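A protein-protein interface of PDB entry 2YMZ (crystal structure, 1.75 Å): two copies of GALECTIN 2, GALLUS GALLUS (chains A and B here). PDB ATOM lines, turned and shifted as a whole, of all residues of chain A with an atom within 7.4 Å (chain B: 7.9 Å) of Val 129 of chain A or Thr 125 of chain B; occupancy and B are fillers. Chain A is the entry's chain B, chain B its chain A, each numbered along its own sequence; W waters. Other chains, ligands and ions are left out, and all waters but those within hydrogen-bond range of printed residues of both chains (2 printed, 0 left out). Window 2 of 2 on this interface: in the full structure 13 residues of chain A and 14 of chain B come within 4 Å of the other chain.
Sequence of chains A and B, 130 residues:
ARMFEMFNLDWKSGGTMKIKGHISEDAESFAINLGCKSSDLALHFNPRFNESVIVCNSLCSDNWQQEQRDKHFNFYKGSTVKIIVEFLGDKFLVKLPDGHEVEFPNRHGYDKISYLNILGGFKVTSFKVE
The backbone NH (N) of Met 6 of chain A is in hydrogen-bond range of the backbone carbonyl oxygen (O) of Leu 116 of chain A (2.9 Å). The backbone NH (N) of Thr 125 of chain B lies within hydrogen-bond range of the backbone carbonyl oxygen (O) of Lys 20 of chain B (2.9 Å). The backbone NH (N) of Lys 20 of chain B lies within hydrogen-bond range of the backbone carbonyl oxygen (O) of Ser 126 of chain B (2.9 Å). O of Lys 128 of chain A is in hydrogen-bond range of N of Lys 18 of chain A.
Water W1 lies within hydrogen-bond range of O of Val 129 of chain A (3.0 Å) and O of Thr 125 of chain B (3.4 Å). Water W2 lies within hydrogen-bond range of the side-chain hydroxyl of Ser 126 of chain B (3.0 Å) and the backbone carbonyl oxygen of Phe 127 of chain A (3.1 Å).
Phe 127 of chain B touches its own counterpart, Phe 127 of chain A. Of the 6 pairs that touch across the chains among the printed residues, 1 has its exchanged pair printed and touching as well.
The backbone carbonyl oxygen (O) of Phe 127 of chain B sits at hydrogen-bond distance from the backbone NH (N) of Phe 127 of chain A, 2.8 Å away. The backbone carbonyl oxygen (O) of Thr 125 of chain B is in hydrogen-bond range of the backbone NH (N) of Val 129 of chain A (2.9 Å).
Of chain B, only Val 124 (3.8 Å) and Thr 125 (2.9 Å) come within 4 Å of Val 129 of chain A. Of chain A, only Lys 128 (3.3 Å) and Val 129 (2.9 Å) come within 4 Å of Thr 125 of chain B. Printed residues of chain B within 4 Å of Lys 128 of chain A: Thr 125 (3.3 Å). Printed residues of chain A within 4 Å of Ser 126 of chain B: Phe 127. Leu 116 of chain A touches none of the printed residues of chain B. The nearest residue of chain B that does not touch Val 129 of chain A is Ser 126 of chain B (5.1 Å). The nearest printed residue of chain A that does not touch Val 124 of chain B is Phe 127 of chain A (4.6 Å).
Hydrophobic or aromatic side chains of chain A that line the printed part of chain B: Met 6 and Val 129. Of the 15 printed residues of chain B, 5 touch a printed residue of chain A. Hydrophobic or aromatic side chains of chain B that line the printed part of chain A: Phe 4. Among the printed residues, 6 pairs touch across the chains. Among the printed residues, no Asp or Glu carboxylate lies within 4 Å of a Lys or Arg side-chain nitrogen of the other chain.
Among the printed residues, merely in contact across the chains: Phe 127 of chain A with Ser 126 of chain B, Met 6 of chain A with Phe 4 of chain B, Lys 128 of chain A with Thr 125 of chain B and Val 129 of chain A with Val 124 of chain B.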
ATOM      1  N   MET A   6     -20.933  31.149 -33.430  1.00  0.00           N
ATOM      2  CA  MET A   6     -19.705  30.408 -33.373  1.00  0.00           C
ATOM      3  C   MET A   6     -19.580  29.511 -34.583  1.00  0.00           C
ATOM      4  O   MET A   6     -20.567  28.926 -35.048  1.00  0.00           O
ATOM      5  CB  MET A   6     -19.714  29.573 -32.091  1.00  0.00           C
ATOM      6  CG  MET A   6     -18.364  29.119 -31.687  1.00  0.00           C
ATOM      7  SD  MET A   6     -18.646  28.293 -30.135  1.00  0.00           S
ATOM      8  CE  MET A   6     -19.160  29.569 -28.974  1.00  0.00           C
ATOM      9  N   LEU A   9     -17.219  24.736 -34.393  1.00  0.00           N
ATOM     10  CA  LEU A   9     -17.526  24.015 -33.125  1.00  0.00           C
ATOM     11  C   LEU A   9     -16.971  22.609 -32.970  1.00  0.00           C
ATOM     12  O   LEU A   9     -16.698  22.172 -31.866  1.00  0.00           O
ATOM     13  CB  LEU A   9     -19.036  23.860 -32.922  1.00  0.00           C
ATOM     14  CG  LEU A   9     -19.722  24.973 -32.142  1.00  0.00           C
ATOM     15  CD1 LEU A   9     -21.207  24.684 -32.103  1.00  0.00           C
ATOM     16  CD2 LEU A   9     -19.111  25.168 -30.753  1.00  0.00           C
ATOM     17  N   ASP A  10     -16.935  21.872 -34.051  1.00  0.00           N
ATOM     18  CA  ASP A  10     -16.563  20.443 -33.979  1.00  0.00           C
ATOM     19  C   ASP A  10     -17.288  19.665 -32.864  1.00  0.00           C
ATOM     20  O   ASP A  10     -16.673  18.924 -32.084  1.00  0.00           O
ATOM     21  CB  ASP A  10     -15.024  20.313 -33.837  1.00  0.00           C
ATOM     22  CG  ASP A  10     -14.503  18.923 -34.151  1.00  0.00           C
ATOM     23  OD1 ASP A  10     -15.172  18.135 -34.881  1.00  0.00           O
ATOM     24  OD2 ASP A  10     -13.376  18.631 -33.655  1.00  0.00           O
ATOM     25  N   TRP A  11     -18.598  19.827 -32.791  1.00  0.00           N
ATOM     26  CA  TRP A  11     -19.369  19.190 -31.746  1.00  0.00           C
ATOM     27  C   TRP A  11     -19.975  17.905 -32.305  1.00  0.00           C
ATOM     28  O   TRP A  11     -20.551  17.847 -33.415  1.00  0.00           O
ATOM     29  CB  TRP A  11     -20.513  20.112 -31.349  1.00  0.00           C
ATOM     30  CG  TRP A  11     -21.226  19.743 -30.081  1.00  0.00           C
ATOM     31  CD1 TRP A  11     -20.657  19.331 -28.903  1.00  0.00           C
ATOM     32  CD2 TRP A  11     -22.611  19.814 -29.865  1.00  0.00           C
ATOM     33  NE1 TRP A  11     -21.650  19.164 -27.947  1.00  0.00           N
ATOM     34  CE2 TRP A  11     -22.854  19.431 -28.506  1.00  0.00           C
ATOM     35  CE3 TRP A  11     -23.703  20.142 -30.681  1.00  0.00           C
ATOM     36  CZ2 TRP A  11     -24.138  19.357 -27.950  1.00  0.00           C
ATOM     37  CZ3 TRP A  11     -25.032  20.050 -30.104  1.00  0.00           C
ATOM     38  CH2 TRP A  11     -25.216  19.680 -28.733  1.00  0.00           C
ATOM     39  N   LYS A  12     -19.775  16.830 -31.588  1.00  0.00           N
ATOM     40  CA  LYS A  12     -20.054  15.501 -32.192  1.00  0.00           C
ATOM     41  C   LYS A  12     -21.001  14.714 -31.321  1.00  0.00           C
ATOM     42  O   LYS A  12     -21.246  15.063 -30.159  1.00  0.00           O
ATOM     43  CB  LYS A  12     -18.731  14.722 -32.358  1.00  0.00           C
ATOM     44  CG  LYS A  12     -17.688  15.345 -33.267  1.00  0.00           C
ATOM     45  CD  LYS A  12     -16.436  14.438 -33.331  1.00  0.00           C
ATOM     46  CE  LYS A  12     -15.520  14.789 -34.510  1.00  0.00           C
ATOM     47  NZ  LYS A  12     -14.074  14.843 -34.124  1.00  0.00           N
ATOM     48  N   GLY A  15     -21.963  14.608 -27.384  1.00  0.00           N
ATOM     49  CA  GLY A  15     -21.592  15.906 -26.794  1.00  0.00           C
ATOM     50  C   GLY A  15     -22.738  16.558 -26.039  1.00  0.00           C
ATOM     51  O   GLY A  15     -23.915  16.227 -26.223  1.00  0.00           O
ATOM     52  N   THR A  16     -22.375  17.503 -25.157  1.00  0.00           N
ATOM     53  CA  THR A  16     -23.301  18.199 -24.298  1.00  0.00           C
ATOM     54  C   THR A  16     -22.953  19.697 -24.441  1.00  0.00           C
ATOM     55  O   THR A  16     -21.790  20.093 -24.649  1.00  0.00           O
ATOM     56  CB  THR A  16     -23.088  17.820 -22.808  1.00  0.00           C
ATOM     57  OG1 THR A  16     -23.381  16.429 -22.630  1.00  0.00           O
ATOM     58  CG2 THR A  16     -24.093  18.536 -21.958  1.00  0.00           C
ATOM     59  N   MET A  17     -23.988  20.524 -24.485  1.00  0.00           N
ATOM     60  CA  MET A  17     -23.739  21.998 -24.569  1.00  0.00           C
ATOM     61  C   MET A  17     -24.639  22.627 -23.465  1.00  0.00           C
ATOM     62  O   MET A  17     -25.831  22.293 -23.353  1.00  0.00           O
ATOM     63  CB  MET A  17     -24.141  22.484 -25.994  1.00  0.00           C
ATOM     64  CG  MET A  17     -23.978  23.975 -26.153  1.00  0.00           C
ATOM     65  SD  MET A  17     -24.403  24.466 -27.881  1.00  0.00           S
ATOM     66  CE  MET A  17     -23.137  23.674 -28.886  1.00  0.00           C
ATOM     67  N   LYS A  18     -24.096  23.576 -22.720  1.00  0.00           N
ATOM     68  CA  LYS A  18     -24.855  24.251 -21.733  1.00  0.00           C
ATOM     69  C   LYS A  18     -24.919  25.718 -22.229  1.00  0.00           C
ATOM     70  O   LYS A  18     -23.897  26.326 -22.533  1.00  0.00           O
ATOM     71  CB  LYS A  18     -24.070  24.233 -20.402  1.00  0.00           C
ATOM     72  CG  LYS A  18     -24.773  25.115 -19.331  1.00  0.00           C
ATOM     73  CD  LYS A  18     -23.829  26.105 -18.646  1.00  0.00           C
ATOM     74  CE  LYS A  18     -22.955  25.400 -17.637  1.00  0.00           C
ATOM     75  NZ  LYS A  18     -22.605  26.388 -16.596  1.00  0.00           N
ATOM     76  N   ILE A 113     -21.510  18.892 -35.627  1.00  0.00           N
ATOM     77  CA  ILE A 113     -22.182  20.208 -35.762  1.00  0.00           C
ATOM     78  C   ILE A 113     -21.109  21.249 -35.649  1.00  0.00           C
ATOM     79  O   ILE A 113     -20.326  21.218 -34.679  1.00  0.00           O
ATOM     80  CB  ILE A 113     -23.223  20.406 -34.620  1.00  0.00           C
ATOM     81  CG1 ILE A 113     -24.460  19.520 -34.779  1.00  0.00           C
ATOM     82  CG2 ILE A 113     -23.586  21.890 -34.366  1.00  0.00           C
ATOM     83  CD1 ILE A 113     -25.349  19.828 -35.939  1.00  0.00           C
ATOM     84  N   LEU A 116     -23.146  27.418 -34.491  1.00  0.00           N
ATOM     85  CA  LEU A 116     -24.194  27.751 -33.466  1.00  0.00           C
ATOM     86  C   LEU A 116     -24.482  29.295 -33.628  1.00  0.00           C
ATOM     87  O   LEU A 116     -23.563  30.096 -33.782  1.00  0.00           O
ATOM     88  CB  LEU A 116     -23.561  27.625 -32.060  1.00  0.00           C
ATOM     89  CG  LEU A 116     -24.346  28.233 -30.829  1.00  0.00           C
ATOM     90  CD1 LEU A 116     -25.773  27.695 -30.617  1.00  0.00           C
ATOM     91  CD2 LEU A 116     -23.562  28.105 -29.539  1.00  0.00           C
ATOM     92  N   PHE A 127     -21.613  29.720 -21.189  1.00  0.00           N
ATOM     93  CA  PHE A 127     -21.719  28.749 -22.317  1.00  0.00           C
ATOM     94  C   PHE A 127     -20.643  27.687 -22.063  1.00  0.00           C
ATOM     95  O   PHE A 127     -19.493  28.035 -21.745  1.00  0.00           O
ATOM     96  CB  PHE A 127     -21.317  29.490 -23.619  1.00  0.00           C
ATOM     97  CG  PHE A 127     -21.095  28.571 -24.800  1.00  0.00           C
ATOM     98  CD1 PHE A 127     -22.149  27.884 -25.367  1.00  0.00           C
ATOM     99  CD2 PHE A 127     -19.803  28.370 -25.274  1.00  0.00           C
ATOM    100  CE1 PHE A 127     -21.936  27.079 -26.503  1.00  0.00           C
ATOM    101  CE2 PHE A 127     -19.583  27.483 -26.335  1.00  0.00           C
ATOM    102  CZ  PHE A 127     -20.649  26.885 -26.965  1.00  0.00           C
ATOM    103  N   LYS A 128     -20.944  26.413 -22.343  1.00  0.00           N
ATOM    104  CA  LYS A 128     -19.890  25.401 -22.245  1.00  0.00           C
ATOM    105  C   LYS A 128     -20.220  24.346 -23.293  1.00  0.00           C
ATOM    106  O   LYS A 128     -21.396  23.985 -23.501  1.00  0.00           O
ATOM    107  CB  LYS A 128     -19.920  24.763 -20.837  1.00  0.00           C
ATOM    108  CG  LYS A 128     -18.816  23.688 -20.630  1.00  0.00           C
ATOM    109  CD  LYS A 128     -19.018  23.120 -19.223  1.00  0.00           C
ATOM    110  CE  LYS A 128     -17.741  22.535 -18.626  1.00  0.00           C
ATOM    111  NZ  LYS A 128     -18.032  22.239 -17.179  1.00  0.00           N
ATOM    112  N   VAL A 129     -19.213  23.823 -23.990  1.00  0.00           N
ATOM    113  CA  VAL A 129     -19.495  22.773 -24.972  1.00  0.00           C
ATOM    114  C   VAL A 129     -18.432  21.676 -24.765  1.00  0.00           C
ATOM    115  O   VAL A 129     -17.225  21.984 -24.555  1.00  0.00           O
ATOM    116  CB  VAL A 129     -19.511  23.311 -26.456  1.00  0.00           C
ATOM    117  CG1 VAL A 129     -18.213  24.062 -26.770  1.00  0.00           C
ATOM    118  CG2 VAL A 129     -19.719  22.145 -27.494  1.00  0.00           C
ATOM    119  N   GLU A 130     -18.882  20.418 -24.772  1.00  0.00           N
ATOM    120  CA  GLU A 130     -17.926  19.338 -24.715  1.00  0.00           C
ATOM    121  C   GLU A 130     -18.396  18.198 -25.573  1.00  0.00           C
ATOM    122  O   GLU A 130     -19.531  18.165 -26.040  1.00  0.00           O
ATOM    123  CB  GLU A 130     -17.777  18.948 -23.251  1.00  0.00           C
ATOM    124  CG  GLU A 130     -19.040  18.325 -22.754  1.00  0.00           C
ATOM    125  CD  GLU A 130     -19.057  18.132 -21.242  1.00  0.00           C
ATOM    126  OE1 GLU A 130     -18.292  18.840 -20.509  1.00  0.00           O
ATOM    127  OE2 GLU A 130     -19.845  17.244 -20.826  1.00  0.00           O
ATOM    128  OXT GLU A 130     -17.600  17.283 -25.809  1.00  0.00           O
ATOM    129  N   PHE B   4     -15.629  33.038 -32.859  1.00  0.00           N
ATOM    130  CA  PHE B   4     -16.657  33.292 -31.880  1.00  0.00           C
ATOM    131  C   PHE B   4     -16.956  34.799 -32.006  1.00  0.00           C
ATOM    132  O   PHE B   4     -16.043  35.625 -32.061  1.00  0.00           O
ATOM    133  CB  PHE B   4     -15.970  32.931 -30.579  1.00  0.00           C
ATOM    134  CG  PHE B   4     -16.736  33.124 -29.329  1.00  0.00           C
ATOM    135  CD1 PHE B   4     -16.853  34.373 -28.735  1.00  0.00           C
ATOM    136  CD2 PHE B   4     -17.175  32.016 -28.624  1.00  0.00           C
ATOM    137  CE1 PHE B   4     -17.509  34.515 -27.527  1.00  0.00           C
ATOM    138  CE2 PHE B   4     -17.839  32.169 -27.400  1.00  0.00           C
ATOM    139  CZ  PHE B   4     -17.999  33.428 -26.865  1.00  0.00           C
ATOM    140  N   LYS B  18     -14.630  34.976 -18.212  1.00  0.00           N
ATOM    141  CA  LYS B  18     -13.798  33.769 -18.077  1.00  0.00           C
ATOM    142  C   LYS B  18     -13.903  33.076 -19.421  1.00  0.00           C
ATOM    143  O   LYS B  18     -15.017  32.759 -19.904  1.00  0.00           O
ATOM    144  CB  LYS B  18     -14.321  32.907 -16.898  1.00  0.00           C
ATOM    145  CG  LYS B  18     -14.119  33.705 -15.594  1.00  0.00           C
ATOM    146  CD  LYS B  18     -14.824  33.059 -14.384  1.00  0.00           C
ATOM    147  CE  LYS B  18     -15.172  34.128 -13.333  1.00  0.00           C
ATOM    148  NZ  LYS B  18     -15.968  33.535 -12.223  1.00  0.00           N
ATOM    149  N   ILE B  19     -12.743  32.894 -20.083  1.00  0.00           N
ATOM    150  CA  ILE B  19     -12.725  32.297 -21.398  1.00  0.00           C
ATOM    151  C   ILE B  19     -11.813  31.078 -21.290  1.00  0.00           C
ATOM    152  O   ILE B  19     -10.632  31.237 -21.015  1.00  0.00           O
ATOM    153  CB  ILE B  19     -12.134  33.294 -22.414  1.00  0.00           C
ATOM    154  CG1 ILE B  19     -13.147  34.433 -22.645  1.00  0.00           C
ATOM    155  CG2 ILE B  19     -11.899  32.608 -23.790  1.00  0.00           C
ATOM    156  CD1 ILE B  19     -12.585  35.672 -23.332  1.00  0.00           C
ATOM    157  N   LYS B  20     -12.315  29.902 -21.565  1.00  0.00           N
ATOM    158  CA  LYS B  20     -11.452  28.720 -21.592  1.00  0.00           C
ATOM    159  C   LYS B  20     -11.512  28.170 -22.927  1.00  0.00           C
ATOM    160  O   LYS B  20     -12.564  28.169 -23.580  1.00  0.00           O
ATOM    161  CB  LYS B  20     -11.928  27.559 -20.697  1.00  0.00           C
ATOM    162  CG  LYS B  20     -11.942  27.814 -19.235  1.00  0.00           C
ATOM    163  CD  LYS B  20     -12.379  26.476 -18.567  1.00  0.00           C
ATOM    164  CE  LYS B  20     -11.191  25.590 -18.292  1.00  0.00           C
ATOM    165  NZ  LYS B  20     -11.594  24.526 -17.275  1.00  0.00           N
ATOM    166  N   GLY B  21     -10.396  27.609 -23.409  1.00  0.00           N
ATOM    167  CA  GLY B  21     -10.486  27.020 -24.715  1.00  0.00           C
ATOM    168  C   GLY B  21      -9.213  26.323 -25.099  1.00  0.00           C
ATOM    169  O   GLY B  21      -8.246  26.294 -24.292  1.00  0.00           O
ATOM    170  N   HIS B  22      -9.281  25.677 -26.252  1.00  0.00           N
ATOM    171  CA  HIS B  22      -8.164  24.863 -26.758  1.00  0.00           C
ATOM    172  C   HIS B  22      -7.291  25.644 -27.781  1.00  0.00           C
ATOM    173  O   HIS B  22      -7.791  26.113 -28.794  1.00  0.00           O
ATOM    174  CB  HIS B  22      -8.757  23.633 -27.420  1.00  0.00           C
ATOM    175  CG  HIS B  22      -7.693  22.694 -27.914  1.00  0.00           C
ATOM    176  ND1 HIS B  22      -6.977  21.860 -27.083  1.00  0.00           N
ATOM    177  CD2 HIS B  22      -7.184  22.523 -29.152  1.00  0.00           C
ATOM    178  CE1 HIS B  22      -6.076  21.199 -27.804  1.00  0.00           C
ATOM    179  NE2 HIS B  22      -6.177  21.589 -29.055  1.00  0.00           N
ATOM    180  N   ILE B  23      -5.979  25.691 -27.532  1.00  0.00           N
ATOM    181  CA  ILE B  23      -5.056  26.351 -28.490  1.00  0.00           C
ATOM    182  C   ILE B  23      -4.664  25.259 -29.471  1.00  0.00           C
ATOM    183  O   ILE B  23      -4.249  24.222 -29.051  1.00  0.00           O
ATOM    184  CB  ILE B  23      -3.825  26.879 -27.749  1.00  0.00           C
ATOM    185  CG1 ILE B  23      -4.276  28.012 -26.756  1.00  0.00           C
ATOM    186  CG2 ILE B  23      -2.787  27.477 -28.736  1.00  0.00           C
ATOM    187  CD1 ILE B  23      -3.207  28.444 -25.752  1.00  0.00           C
ATOM    188  N   THR B  80      -5.301  23.252 -23.253  1.00  0.00           N
ATOM    189  CA  THR B  80      -6.581  23.946 -22.902  1.00  0.00           C
ATOM    190  C   THR B  80      -6.224  24.936 -21.836  1.00  0.00           C
ATOM    191  O   THR B  80      -5.428  24.589 -20.954  1.00  0.00           O
ATOM    192  CB  THR B  80      -7.589  22.956 -22.323  1.00  0.00           C
ATOM    193  OG1 THR B  80      -8.035  22.140 -23.382  1.00  0.00           O
ATOM    194  CG2 THR B  80      -8.852  23.661 -21.695  1.00  0.00           C
ATOM    195  N   VAL B  81      -6.650  26.197 -21.981  1.00  0.00           N
ATOM    196  CA  VAL B  81      -6.225  27.249 -21.052  1.00  0.00           C
ATOM    197  C   VAL B  81      -7.410  28.078 -20.629  1.00  0.00           C
ATOM    198  O   VAL B  81      -8.390  28.176 -21.381  1.00  0.00           O
ATOM    199  CB  VAL B  81      -5.206  28.252 -21.624  1.00  0.00           C
ATOM    200  CG1 VAL B  81      -3.895  27.551 -21.847  1.00  0.00           C
ATOM    201  CG2 VAL B  81      -5.673  28.954 -22.905  1.00  0.00           C
ATOM    202  N   PHE B 122      -7.726  29.283 -31.487  1.00  0.00           N
ATOM    203  CA  PHE B 122      -8.260  29.133 -30.165  1.00  0.00           C
ATOM    204  C   PHE B 122      -9.737  28.735 -30.329  1.00  0.00           C
ATOM    205  O   PHE B 122     -10.492  29.471 -30.968  1.00  0.00           O
ATOM    206  CB  PHE B 122      -8.108  30.436 -29.363  1.00  0.00           C
ATOM    207  CG  PHE B 122      -8.492  30.325 -27.936  1.00  0.00           C
ATOM    208  CD1 PHE B 122      -9.814  30.480 -27.534  1.00  0.00           C
ATOM    209  CD2 PHE B 122      -7.526  30.038 -26.946  1.00  0.00           C
ATOM    210  CE1 PHE B 122     -10.171  30.373 -26.214  1.00  0.00           C
ATOM    211  CE2 PHE B 122      -7.885  29.956 -25.602  1.00  0.00           C
ATOM    212  CZ  PHE B 122      -9.199  30.104 -25.216  1.00  0.00           C
ATOM    213  N   LYS B 123     -10.108  27.546 -29.857  1.00  0.00           N
ATOM    214  CA  LYS B 123     -11.494  27.053 -29.961  1.00  0.00           C
ATOM    215  C   LYS B 123     -12.100  27.197 -28.558  1.00  0.00           C
ATOM    216  O   LYS B 123     -11.647  26.530 -27.630  1.00  0.00           O
ATOM    217  CB  LYS B 123     -11.631  25.551 -30.336  1.00  0.00           C
ATOM    218  CG  LYS B 123     -10.911  25.054 -31.583  1.00  0.00           C
ATOM    219  CD  LYS B 123     -11.567  25.382 -32.923  1.00  0.00           C
ATOM    220  CE  LYS B 123     -10.515  25.544 -34.043  1.00  0.00           C
ATOM    221  NZ  LYS B 123     -10.175  24.251 -34.687  1.00  0.00           N
ATOM    222  N   VAL B 124     -13.127  28.047 -28.394  1.00  0.00           N
ATOM    223  CA  VAL B 124     -13.711  28.270 -27.084  1.00  0.00           C
ATOM    224  C   VAL B 124     -14.442  27.016 -26.576  1.00  0.00           C
ATOM    225  O   VAL B 124     -15.259  26.415 -27.280  1.00  0.00           O
ATOM    226  CB  VAL B 124     -14.701  29.495 -27.122  1.00  0.00           C
ATOM    227  CG1 VAL B 124     -15.441  29.654 -25.789  1.00  0.00           C
ATOM    228  CG2 VAL B 124     -13.893  30.761 -27.471  1.00  0.00           C
ATOM    229  N   THR B 125     -14.111  26.565 -25.382  1.00  0.00           N
ATOM    230  CA  THR B 125     -14.905  25.509 -24.759  1.00  0.00           C
ATOM    231  C   THR B 125     -15.783  25.953 -23.589  1.00  0.00           C
ATOM    232  O   THR B 125     -16.773  25.301 -23.314  1.00  0.00           O
ATOM    233  CB  THR B 125     -13.995  24.334 -24.274  1.00  0.00           C
ATOM    234  OG1 THR B 125     -13.088  24.846 -23.379  1.00  0.00           O
ATOM    235  CG2 THR B 125     -13.174  23.765 -25.401  1.00  0.00           C
ATOM    236  N   SER B 126     -15.475  27.060 -22.929  1.00  0.00           N
ATOM    237  CA  SER B 126     -16.362  27.572 -21.850  1.00  0.00           C
ATOM    238  C   SER B 126     -16.249  29.105 -21.904  1.00  0.00           C
ATOM    239  O   SER B 126     -15.159  29.640 -22.176  1.00  0.00           O
ATOM    240  CB  SER B 126     -15.798  27.074 -20.490  1.00  0.00           C
ATOM    241  OG  SER B 126     -16.616  27.408 -19.397  1.00  0.00           O
ATOM    242  N   PHE B 127     -17.351  29.817 -21.634  1.00  0.00           N
ATOM    243  CA  PHE B 127     -17.325  31.278 -21.616  1.00  0.00           C
ATOM    244  C   PHE B 127     -18.273  31.675 -20.492  1.00  0.00           C
ATOM    245  O   PHE B 127     -19.363  31.135 -20.419  1.00  0.00           O
ATOM    246  CB  PHE B 127     -17.834  31.800 -22.959  1.00  0.00           C
ATOM    247  CG  PHE B 127     -18.209  33.247 -22.939  1.00  0.00           C
ATOM    248  CD1 PHE B 127     -17.218  34.236 -23.067  1.00  0.00           C
ATOM    249  CD2 PHE B 127     -19.566  33.619 -22.802  1.00  0.00           C
ATOM    250  CE1 PHE B 127     -17.590  35.613 -23.013  1.00  0.00           C
ATOM    251  CE2 PHE B 127     -19.908  34.954 -22.752  1.00  0.00           C
ATOM    252  CZ  PHE B 127     -18.931  35.941 -22.890  1.00  0.00           C
HETATM  253  O   HOH W   1     -16.132  22.346 -21.761  1.00  0.00           O
HETATM  254  O   HOH W   2     -19.476  28.068 -18.650  1.00  0.00           O
